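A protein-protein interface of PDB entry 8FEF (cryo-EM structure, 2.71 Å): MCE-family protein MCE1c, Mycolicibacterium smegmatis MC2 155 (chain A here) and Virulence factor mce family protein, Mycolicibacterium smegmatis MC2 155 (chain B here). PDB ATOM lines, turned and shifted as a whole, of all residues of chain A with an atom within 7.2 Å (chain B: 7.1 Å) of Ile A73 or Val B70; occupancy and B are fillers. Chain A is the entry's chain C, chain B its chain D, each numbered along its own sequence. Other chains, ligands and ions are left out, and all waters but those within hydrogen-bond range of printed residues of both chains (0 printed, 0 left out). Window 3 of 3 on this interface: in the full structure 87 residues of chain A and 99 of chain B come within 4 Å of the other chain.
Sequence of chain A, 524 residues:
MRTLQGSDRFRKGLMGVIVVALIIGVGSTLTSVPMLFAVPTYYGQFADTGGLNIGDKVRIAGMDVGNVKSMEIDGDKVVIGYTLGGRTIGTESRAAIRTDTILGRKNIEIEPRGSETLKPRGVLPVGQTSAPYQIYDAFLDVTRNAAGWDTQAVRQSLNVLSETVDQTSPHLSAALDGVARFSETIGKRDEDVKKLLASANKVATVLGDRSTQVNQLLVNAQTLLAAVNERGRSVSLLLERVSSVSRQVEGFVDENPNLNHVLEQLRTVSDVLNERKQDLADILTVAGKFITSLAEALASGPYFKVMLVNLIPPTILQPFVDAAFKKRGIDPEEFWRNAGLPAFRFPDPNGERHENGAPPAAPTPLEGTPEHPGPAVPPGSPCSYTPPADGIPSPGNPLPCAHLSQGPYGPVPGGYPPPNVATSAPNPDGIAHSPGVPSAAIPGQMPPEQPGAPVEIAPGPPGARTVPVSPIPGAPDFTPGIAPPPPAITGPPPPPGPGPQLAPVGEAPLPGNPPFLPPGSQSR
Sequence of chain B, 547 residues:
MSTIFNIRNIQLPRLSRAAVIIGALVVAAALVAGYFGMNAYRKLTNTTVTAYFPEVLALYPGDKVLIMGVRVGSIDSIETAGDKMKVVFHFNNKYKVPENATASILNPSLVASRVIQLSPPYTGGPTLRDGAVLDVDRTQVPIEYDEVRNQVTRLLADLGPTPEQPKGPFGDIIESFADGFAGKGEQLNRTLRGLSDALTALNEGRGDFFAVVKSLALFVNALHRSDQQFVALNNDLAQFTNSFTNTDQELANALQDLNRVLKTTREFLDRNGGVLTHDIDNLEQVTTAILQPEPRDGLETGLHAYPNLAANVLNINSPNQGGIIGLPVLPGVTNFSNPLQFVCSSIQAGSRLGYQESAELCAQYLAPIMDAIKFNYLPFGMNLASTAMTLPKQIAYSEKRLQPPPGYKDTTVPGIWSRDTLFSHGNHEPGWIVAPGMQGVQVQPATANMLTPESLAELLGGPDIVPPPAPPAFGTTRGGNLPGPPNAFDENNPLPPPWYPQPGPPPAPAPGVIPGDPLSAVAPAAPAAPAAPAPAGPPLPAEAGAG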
ATOM      1  N   ASP A  48       8.879  14.636  -3.280  1.00  0.00           N
ATOM      2  CA  ASP A  48       7.738  15.438  -3.694  1.00  0.00           C
ATOM      3  C   ASP A  48       8.223  16.858  -3.941  1.00  0.00           C
ATOM      4  O   ASP A  48       9.186  17.312  -3.319  1.00  0.00           O
ATOM      5  CB  ASP A  48       6.632  15.411  -2.628  1.00  0.00           C
ATOM      6  CG  ASP A  48       5.308  15.978  -3.122  1.00  0.00           C
ATOM      7  OD1 ASP A  48       5.294  17.044  -3.770  1.00  0.00           O
ATOM      8  OD2 ASP A  48       4.265  15.346  -2.851  1.00  0.00           O
ATOM      9  N   THR A  49       7.549  17.552  -4.863  1.00  0.00           N
ATOM     10  CA  THR A  49       7.866  18.959  -5.085  1.00  0.00           C
ATOM     11  C   THR A  49       7.422  19.820  -3.911  1.00  0.00           C
ATOM     12  O   THR A  49       8.077  20.819  -3.596  1.00  0.00           O
ATOM     13  CB  THR A  49       7.216  19.462  -6.372  1.00  0.00           C
ATOM     14  OG1 THR A  49       5.796  19.529  -6.200  1.00  0.00           O
ATOM     15  CG2 THR A  49       7.532  18.535  -7.525  1.00  0.00           C
ATOM     16  N   MET A  71      11.363  20.649 -13.228  1.00  0.00           N
ATOM     17  CA  MET A  71      10.840  19.612 -12.344  1.00  0.00           C
ATOM     18  C   MET A  71      10.275  18.493 -13.203  1.00  0.00           C
ATOM     19  O   MET A  71       9.302  18.705 -13.931  1.00  0.00           O
ATOM     20  CB  MET A  71       9.759  20.162 -11.407  1.00  0.00           C
ATOM     21  CG  MET A  71      10.247  21.201 -10.416  1.00  0.00           C
ATOM     22  SD  MET A  71       8.918  21.832  -9.381  1.00  0.00           S
ATOM     23  CE  MET A  71       7.778  22.412 -10.632  1.00  0.00           C
ATOM     24  N   GLU A  72      10.878  17.308 -13.122  1.00  0.00           N
ATOM     25  CA  GLU A  72      10.451  16.169 -13.922  1.00  0.00           C
ATOM     26  C   GLU A  72      10.209  14.969 -13.019  1.00  0.00           C
ATOM     27  O   GLU A  72      10.741  14.885 -11.912  1.00  0.00           O
ATOM     28  CB  GLU A  72      11.487  15.815 -14.998  1.00  0.00           C
ATOM     29  CG  GLU A  72      11.720  16.909 -16.030  1.00  0.00           C
ATOM     30  CD  GLU A  72      10.532  17.115 -16.950  1.00  0.00           C
ATOM     31  OE1 GLU A  72       9.742  16.164 -17.130  1.00  0.00           O
ATOM     32  OE2 GLU A  72      10.387  18.229 -17.495  1.00  0.00           O
ATOM     33  N   ILE A  73       9.388  14.040 -13.498  1.00  0.00           N
ATOM     34  CA  ILE A  73       9.084  12.811 -12.774  1.00  0.00           C
ATOM     35  C   ILE A  73       9.958  11.693 -13.324  1.00  0.00           C
ATOM     36  O   ILE A  73       9.877  11.359 -14.512  1.00  0.00           O
ATOM     37  CB  ILE A  73       7.595  12.443 -12.888  1.00  0.00           C
ATOM     38  CG1 ILE A  73       6.732  13.426 -12.100  1.00  0.00           C
ATOM     39  CG2 ILE A  73       7.357  11.023 -12.402  1.00  0.00           C
ATOM     40  CD1 ILE A  73       5.258  13.101 -12.151  1.00  0.00           C
ATOM     41  N   ASP A  74      10.795  11.116 -12.466  1.00  0.00           N
ATOM     42  CA  ASP A  74      11.630   9.972 -12.820  1.00  0.00           C
ATOM     43  C   ASP A  74      11.322   8.855 -11.834  1.00  0.00           C
ATOM     44  O   ASP A  74      11.727   8.922 -10.667  1.00  0.00           O
ATOM     45  CB  ASP A  74      13.113  10.339 -12.811  1.00  0.00           C
ATOM     46  CG  ASP A  74      13.498  11.232 -13.975  1.00  0.00           C
ATOM     47  OD1 ASP A  74      12.770  11.234 -14.989  1.00  0.00           O
ATOM     48  OD2 ASP A  74      14.534  11.922 -13.887  1.00  0.00           O
ATOM     49  N   GLY A  75      10.602   7.838 -12.302  1.00  0.00           N
ATOM     50  CA  GLY A  75      10.240   6.725 -11.439  1.00  0.00           C
ATOM     51  C   GLY A  75       9.373   7.187 -10.287  1.00  0.00           C
ATOM     52  O   GLY A  75       8.332   7.826 -10.476  1.00  0.00           O
ATOM     53  N   ASP A  76       9.801   6.862  -9.068  1.00  0.00           N
ATOM     54  CA  ASP A  76       9.110   7.281  -7.859  1.00  0.00           C
ATOM     55  C   ASP A  76       9.707   8.549  -7.260  1.00  0.00           C
ATOM     56  O   ASP A  76       9.451   8.855  -6.091  1.00  0.00           O
ATOM     57  CB  ASP A  76       9.123   6.154  -6.825  1.00  0.00           C
ATOM     58  CG  ASP A  76      10.524   5.674  -6.504  1.00  0.00           C
ATOM     59  OD1 ASP A  76      11.395   5.742  -7.395  1.00  0.00           O
ATOM     60  OD2 ASP A  76      10.751   5.228  -5.361  1.00  0.00           O
ATOM     61  N   LYS A  77      10.499   9.289  -8.033  1.00  0.00           N
ATOM     62  CA  LYS A  77      11.156  10.490  -7.542  1.00  0.00           C
ATOM     63  C   LYS A  77      10.851  11.658  -8.466  1.00  0.00           C
ATOM     64  O   LYS A  77      10.421  11.483  -9.609  1.00  0.00           O
ATOM     65  CB  LYS A  77      12.675  10.304  -7.434  1.00  0.00           C
ATOM     66  CG  LYS A  77      13.104   9.010  -6.766  1.00  0.00           C
ATOM     67  CD  LYS A  77      14.584   8.750  -6.974  1.00  0.00           C
ATOM     68  CE  LYS A  77      14.953   8.829  -8.446  1.00  0.00           C
ATOM     69  NZ  LYS A  77      14.163   7.875  -9.272  1.00  0.00           N
ATOM     70  N   VAL A  78      11.081  12.862  -7.953  1.00  0.00           N
ATOM     71  CA  VAL A  78      11.030  14.083  -8.744  1.00  0.00           C
ATOM     72  C   VAL A  78      12.447  14.622  -8.847  1.00  0.00           C
ATOM     73  O   VAL A  78      13.092  14.897  -7.827  1.00  0.00           O
ATOM     74  CB  VAL A  78      10.089  15.125  -8.123  1.00  0.00           C
ATOM     75  CG1 VAL A  78      10.210  16.441  -8.863  1.00  0.00           C
ATOM     76  CG2 VAL A  78       8.660  14.628  -8.155  1.00  0.00           C
ATOM     77  N   VAL A  79      12.937  14.758 -10.071  1.00  0.00           N
ATOM     78  CA  VAL A  79      14.233  15.371 -10.320  1.00  0.00           C
ATOM     79  C   VAL A  79      14.009  16.859 -10.546  1.00  0.00           C
ATOM     80  O   VAL A  79      13.320  17.259 -11.491  1.00  0.00           O
ATOM     81  CB  VAL A  79      14.943  14.721 -11.516  1.00  0.00           C
ATOM     82  CG1 VAL A  79      16.120  15.570 -11.954  1.00  0.00           C
ATOM     83  CG2 VAL A  79      15.411  13.328 -11.141  1.00  0.00           C
ATOM     84  N   VAL B  65      -4.467  17.826 -12.071  1.00  0.00           N
ATOM     85  CA  VAL B  65      -4.235  16.538 -11.428  1.00  0.00           C
ATOM     86  C   VAL B  65      -2.730  16.367 -11.291  1.00  0.00           C
ATOM     87  O   VAL B  65      -1.986  16.593 -12.251  1.00  0.00           O
ATOM     88  CB  VAL B  65      -4.859  15.383 -12.232  1.00  0.00           C
ATOM     89  CG1 VAL B  65      -4.430  14.042 -11.669  1.00  0.00           C
ATOM     90  CG2 VAL B  65      -6.370  15.501 -12.227  1.00  0.00           C
ATOM     91  N   LEU B  66      -2.279  15.998 -10.096  1.00  0.00           N
ATOM     92  CA  LEU B  66      -0.860  15.958  -9.786  1.00  0.00           C
ATOM     93  C   LEU B  66      -0.404  14.543  -9.459  1.00  0.00           C
ATOM     94  O   LEU B  66      -1.168  13.726  -8.940  1.00  0.00           O
ATOM     95  CB  LEU B  66      -0.520  16.873  -8.603  1.00  0.00           C
ATOM     96  CG  LEU B  66      -0.942  18.339  -8.661  1.00  0.00           C
ATOM     97  CD1 LEU B  66      -0.331  19.093  -7.500  1.00  0.00           C
ATOM     98  CD2 LEU B  66      -0.547  18.975  -9.976  1.00  0.00           C
ATOM     99  N   ILE B  67       0.851  14.265  -9.792  1.00  0.00           N
ATOM    100  CA  ILE B  67       1.580  13.104  -9.301  1.00  0.00           C
ATOM    101  C   ILE B  67       2.868  13.632  -8.691  1.00  0.00           C
ATOM    102  O   ILE B  67       3.685  14.237  -9.396  1.00  0.00           O
ATOM    103  CB  ILE B  67       1.880  12.081 -10.408  1.00  0.00           C
ATOM    104  CG1 ILE B  67       0.587  11.432 -10.898  1.00  0.00           C
ATOM    105  CG2 ILE B  67       2.845  11.025  -9.906  1.00  0.00           C
ATOM    106  CD1 ILE B  67       0.794  10.416 -11.996  1.00  0.00           C
ATOM    107  N   MET B  68       3.032  13.434  -7.380  1.00  0.00           N
ATOM    108  CA  MET B  68       4.183  13.948  -6.630  1.00  0.00           C
ATOM    109  C   MET B  68       4.349  15.455  -6.821  1.00  0.00           C
ATOM    110  O   MET B  68       5.465  15.977  -6.819  1.00  0.00           O
ATOM    111  CB  MET B  68       5.467  13.208  -7.006  1.00  0.00           C
ATOM    112  CG  MET B  68       5.561  11.808  -6.436  1.00  0.00           C
ATOM    113  SD  MET B  68       7.039  10.939  -6.980  1.00  0.00           S
ATOM    114  CE  MET B  68       6.744  10.858  -8.741  1.00  0.00           C
ATOM    115  N   GLY B  69       3.234  16.162  -6.981  1.00  0.00           N
ATOM    116  CA  GLY B  69       3.247  17.597  -7.164  1.00  0.00           C
ATOM    117  C   GLY B  69       3.446  18.070  -8.587  1.00  0.00           C
ATOM    118  O   GLY B  69       3.447  19.285  -8.819  1.00  0.00           O
ATOM    119  N   VAL B  70       3.607  17.162  -9.546  1.00  0.00           N
ATOM    120  CA  VAL B  70       3.834  17.521 -10.942  1.00  0.00           C
ATOM    121  C   VAL B  70       2.539  17.313 -11.715  1.00  0.00           C
ATOM    122  O   VAL B  70       1.899  16.262 -11.587  1.00  0.00           O
ATOM    123  CB  VAL B  70       4.979  16.693 -11.549  1.00  0.00           C
ATOM    124  CG1 VAL B  70       5.221  17.088 -12.995  1.00  0.00           C
ATOM    125  CG2 VAL B  70       6.246  16.861 -10.726  1.00  0.00           C
ATOM    126  N   ARG B  71       2.143  18.316 -12.499  1.00  0.00           N
ATOM    127  CA  ARG B  71       0.919  18.224 -13.285  1.00  0.00           C
ATOM    128  C   ARG B  71       1.014  17.094 -14.301  1.00  0.00           C
ATOM    129  O   ARG B  71       2.001  16.983 -15.033  1.00  0.00           O
ATOM    130  CB  ARG B  71       0.648  19.545 -14.003  1.00  0.00           C
ATOM    131  CG  ARG B  71       0.458  20.738 -13.087  1.00  0.00           C
ATOM    132  CD  ARG B  71       0.150  21.989 -13.895  1.00  0.00           C
ATOM    133  NE  ARG B  71      -0.118  23.145 -13.048  1.00  0.00           N
ATOM    134  CZ  ARG B  71      -0.473  24.339 -13.504  1.00  0.00           C
ATOM    135  NH1 ARG B  71      -0.610  24.572 -14.798  1.00  0.00           N
ATOM    136  NH2 ARG B  71      -0.696  25.324 -12.638  1.00  0.00           N
ATOM    137  N   VAL B  72      -0.021  16.256 -14.350  1.00  0.00           N
ATOM    138  CA  VAL B  72      -0.053  15.128 -15.273  1.00  0.00           C
ATOM    139  C   VAL B  72      -1.380  15.097 -16.019  1.00  0.00           C
ATOM    140  O   VAL B  72      -1.555  14.312 -16.958  1.00  0.00           O
ATOM    141  CB  VAL B  72       0.180  13.795 -14.537  1.00  0.00           C
ATOM    142  CG1 VAL B  72       1.576  13.746 -13.936  1.00  0.00           C
ATOM    143  CG2 VAL B  72      -0.877  13.596 -13.465  1.00  0.00           C
ATOM    144  N   GLY B  73      -2.320  15.942 -15.618  1.00  0.00           N
ATOM    145  CA  GLY B  73      -3.627  15.920 -16.242  1.00  0.00           C
ATOM    146  C   GLY B  73      -4.531  17.002 -15.700  1.00  0.00           C
ATOM    147  O   GLY B  73      -4.069  17.998 -15.142  1.00  0.00           O
ATOM    148  N   TYR B  95       2.411   8.830 -18.120  1.00  0.00           N
ATOM    149  CA  TYR B  95       2.648   8.419 -16.747  1.00  0.00           C
ATOM    150  C   TYR B  95       1.784   7.217 -16.398  1.00  0.00           C
ATOM    151  O   TYR B  95       0.638   7.109 -16.841  1.00  0.00           O
ATOM    152  CB  TYR B  95       2.356   9.572 -15.785  1.00  0.00           C
ATOM    153  CG  TYR B  95       3.009  10.875 -16.182  1.00  0.00           C
ATOM    154  CD1 TYR B  95       4.303  11.174 -15.781  1.00  0.00           C
ATOM    155  CD2 TYR B  95       2.331  11.808 -16.953  1.00  0.00           C
ATOM    156  CE1 TYR B  95       4.905  12.364 -16.141  1.00  0.00           C
ATOM    157  CE2 TYR B  95       2.924  13.000 -17.318  1.00  0.00           C
ATOM    158  CZ  TYR B  95       4.211  13.271 -16.909  1.00  0.00           C
ATOM    159  OH  TYR B  95       4.805  14.458 -17.268  1.00  0.00           O
ATOM    160  N   GLN B 117      -4.413  14.634  -6.316  1.00  0.00           N
ATOM    161  CA  GLN B 117      -3.125  13.961  -6.389  1.00  0.00           C
ATOM    162  C   GLN B 117      -3.317  12.466  -6.193  1.00  0.00           C
ATOM    163  O   GLN B 117      -4.014  12.038  -5.266  1.00  0.00           O
ATOM    164  CB  GLN B 117      -2.152  14.513  -5.348  1.00  0.00           C
ATOM    165  CG  GLN B 117      -0.806  13.815  -5.344  1.00  0.00           C
ATOM    166  CD  GLN B 117       0.269  14.615  -4.641  1.00  0.00           C
ATOM    167  OE1 GLN B 117       0.293  15.842  -4.716  1.00  0.00           O
ATOM    168  NE2 GLN B 117       1.165  13.923  -3.952  1.00  0.00           N
ATOM    169  N   PRO B 121       3.236   6.968  -5.624  1.00  0.00           N
ATOM    170  CA  PRO B 121       3.940   6.974  -6.910  1.00  0.00           C
ATOM    171  C   PRO B 121       4.155   5.563  -7.430  1.00  0.00           C
ATOM    172  O   PRO B 121       4.307   4.607  -6.667  1.00  0.00           O
ATOM    173  CB  PRO B 121       5.271   7.656  -6.582  1.00  0.00           C
ATOM    174  CG  PRO B 121       5.467   7.411  -5.128  1.00  0.00           C
ATOM    175  CD  PRO B 121       4.096   7.429  -4.521  1.00  0.00           C
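N of Thr A49 sits at hydrogen-bond distance from O of Met B68 (3.3 Å). The backbone carbonyl oxygen (O) of Met B68 sits close to the side-chain carboxylate (OD1) of Asp A48 (3.2 Å). O of Asp A76 sits close to SD of Met B68 (3.3 Å).
The side-chain amino group of Lys A77 is in hydrogen-bond range of the backbone carbonyl oxygen of Asp A74, 3.0 Å away. OD1 of Asp A76 is in salt-bridge range of NZ of Lys A77, 3.97 Å away.
Asp A48 touches Gly B69 (OD1 to N, 3.9 Å). OD2 of Asp A48 touches NE2 of Gln B117, at 3.6 Å. Thr A49 touches Gly B69 (OG1 to CA, 3.3 Å). Val B70 touches Thr A49 (CG2 to CG2, 3.8 Å). O of Ile B67 touches CD1 of Ile A73, 3.4 Å away. Met B68 touches Ile A73 (CE to CG2, 3.7 Å). CD1 of Ile A73 touches CB of Val B70 (3.7 Å). O of Gly A75 touches CE of Met B68, 3.8 Å away. Met B68 touches Lys A77. Val A78 touches Met B68 (CG2 to CB, 3.7 Å).
Of the printed residues of chain B, Asp A48 touches Met B68, Gly B69 and Gln B117. Of chain B, only Ile B67 (3.4 Å), Met B68 (3.7 Å) and Val B70 (3.7 Å) come within 4 Å of Ile A73. Printed residues of chain B within 4 Å of Gly A75: Met B68. Of the printed residues of chain B, Lys A77 touches Met B68 (3.8 Å). Of the printed residues of chain A, Ile B67 touches Ile A73. Val B70 touches just these residues of chain A: Thr A49 and Ile A73. The nearest residue of chain B that does not touch Ile A73 is Tyr B95 (4.1 Å). The nearest residue of chain A that does not touch Val B70 is Val A78 (4.2 Å). The nearest printed residue of chain B that does not touch Thr A49 is Ile B67 (6.1 Å).
Of the 11 printed residues of chain A, 7 touch a printed residue of chain B. Hydrophobic or aromatic side chains of chain A that line the printed part of chain B: Ile A73 and Val A78. Hydrophobic or aromatic side chains of chain B within 4 Å of the printed part of chain A: Ile B67, Met B68 and Val B70. Among the printed residues, 13 pairs touch across the chains. Among the printed residues, no Asp or Glu carboxylate lies within 4 Å of a Lys or Arg side-chain nitrogen of the other chain.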
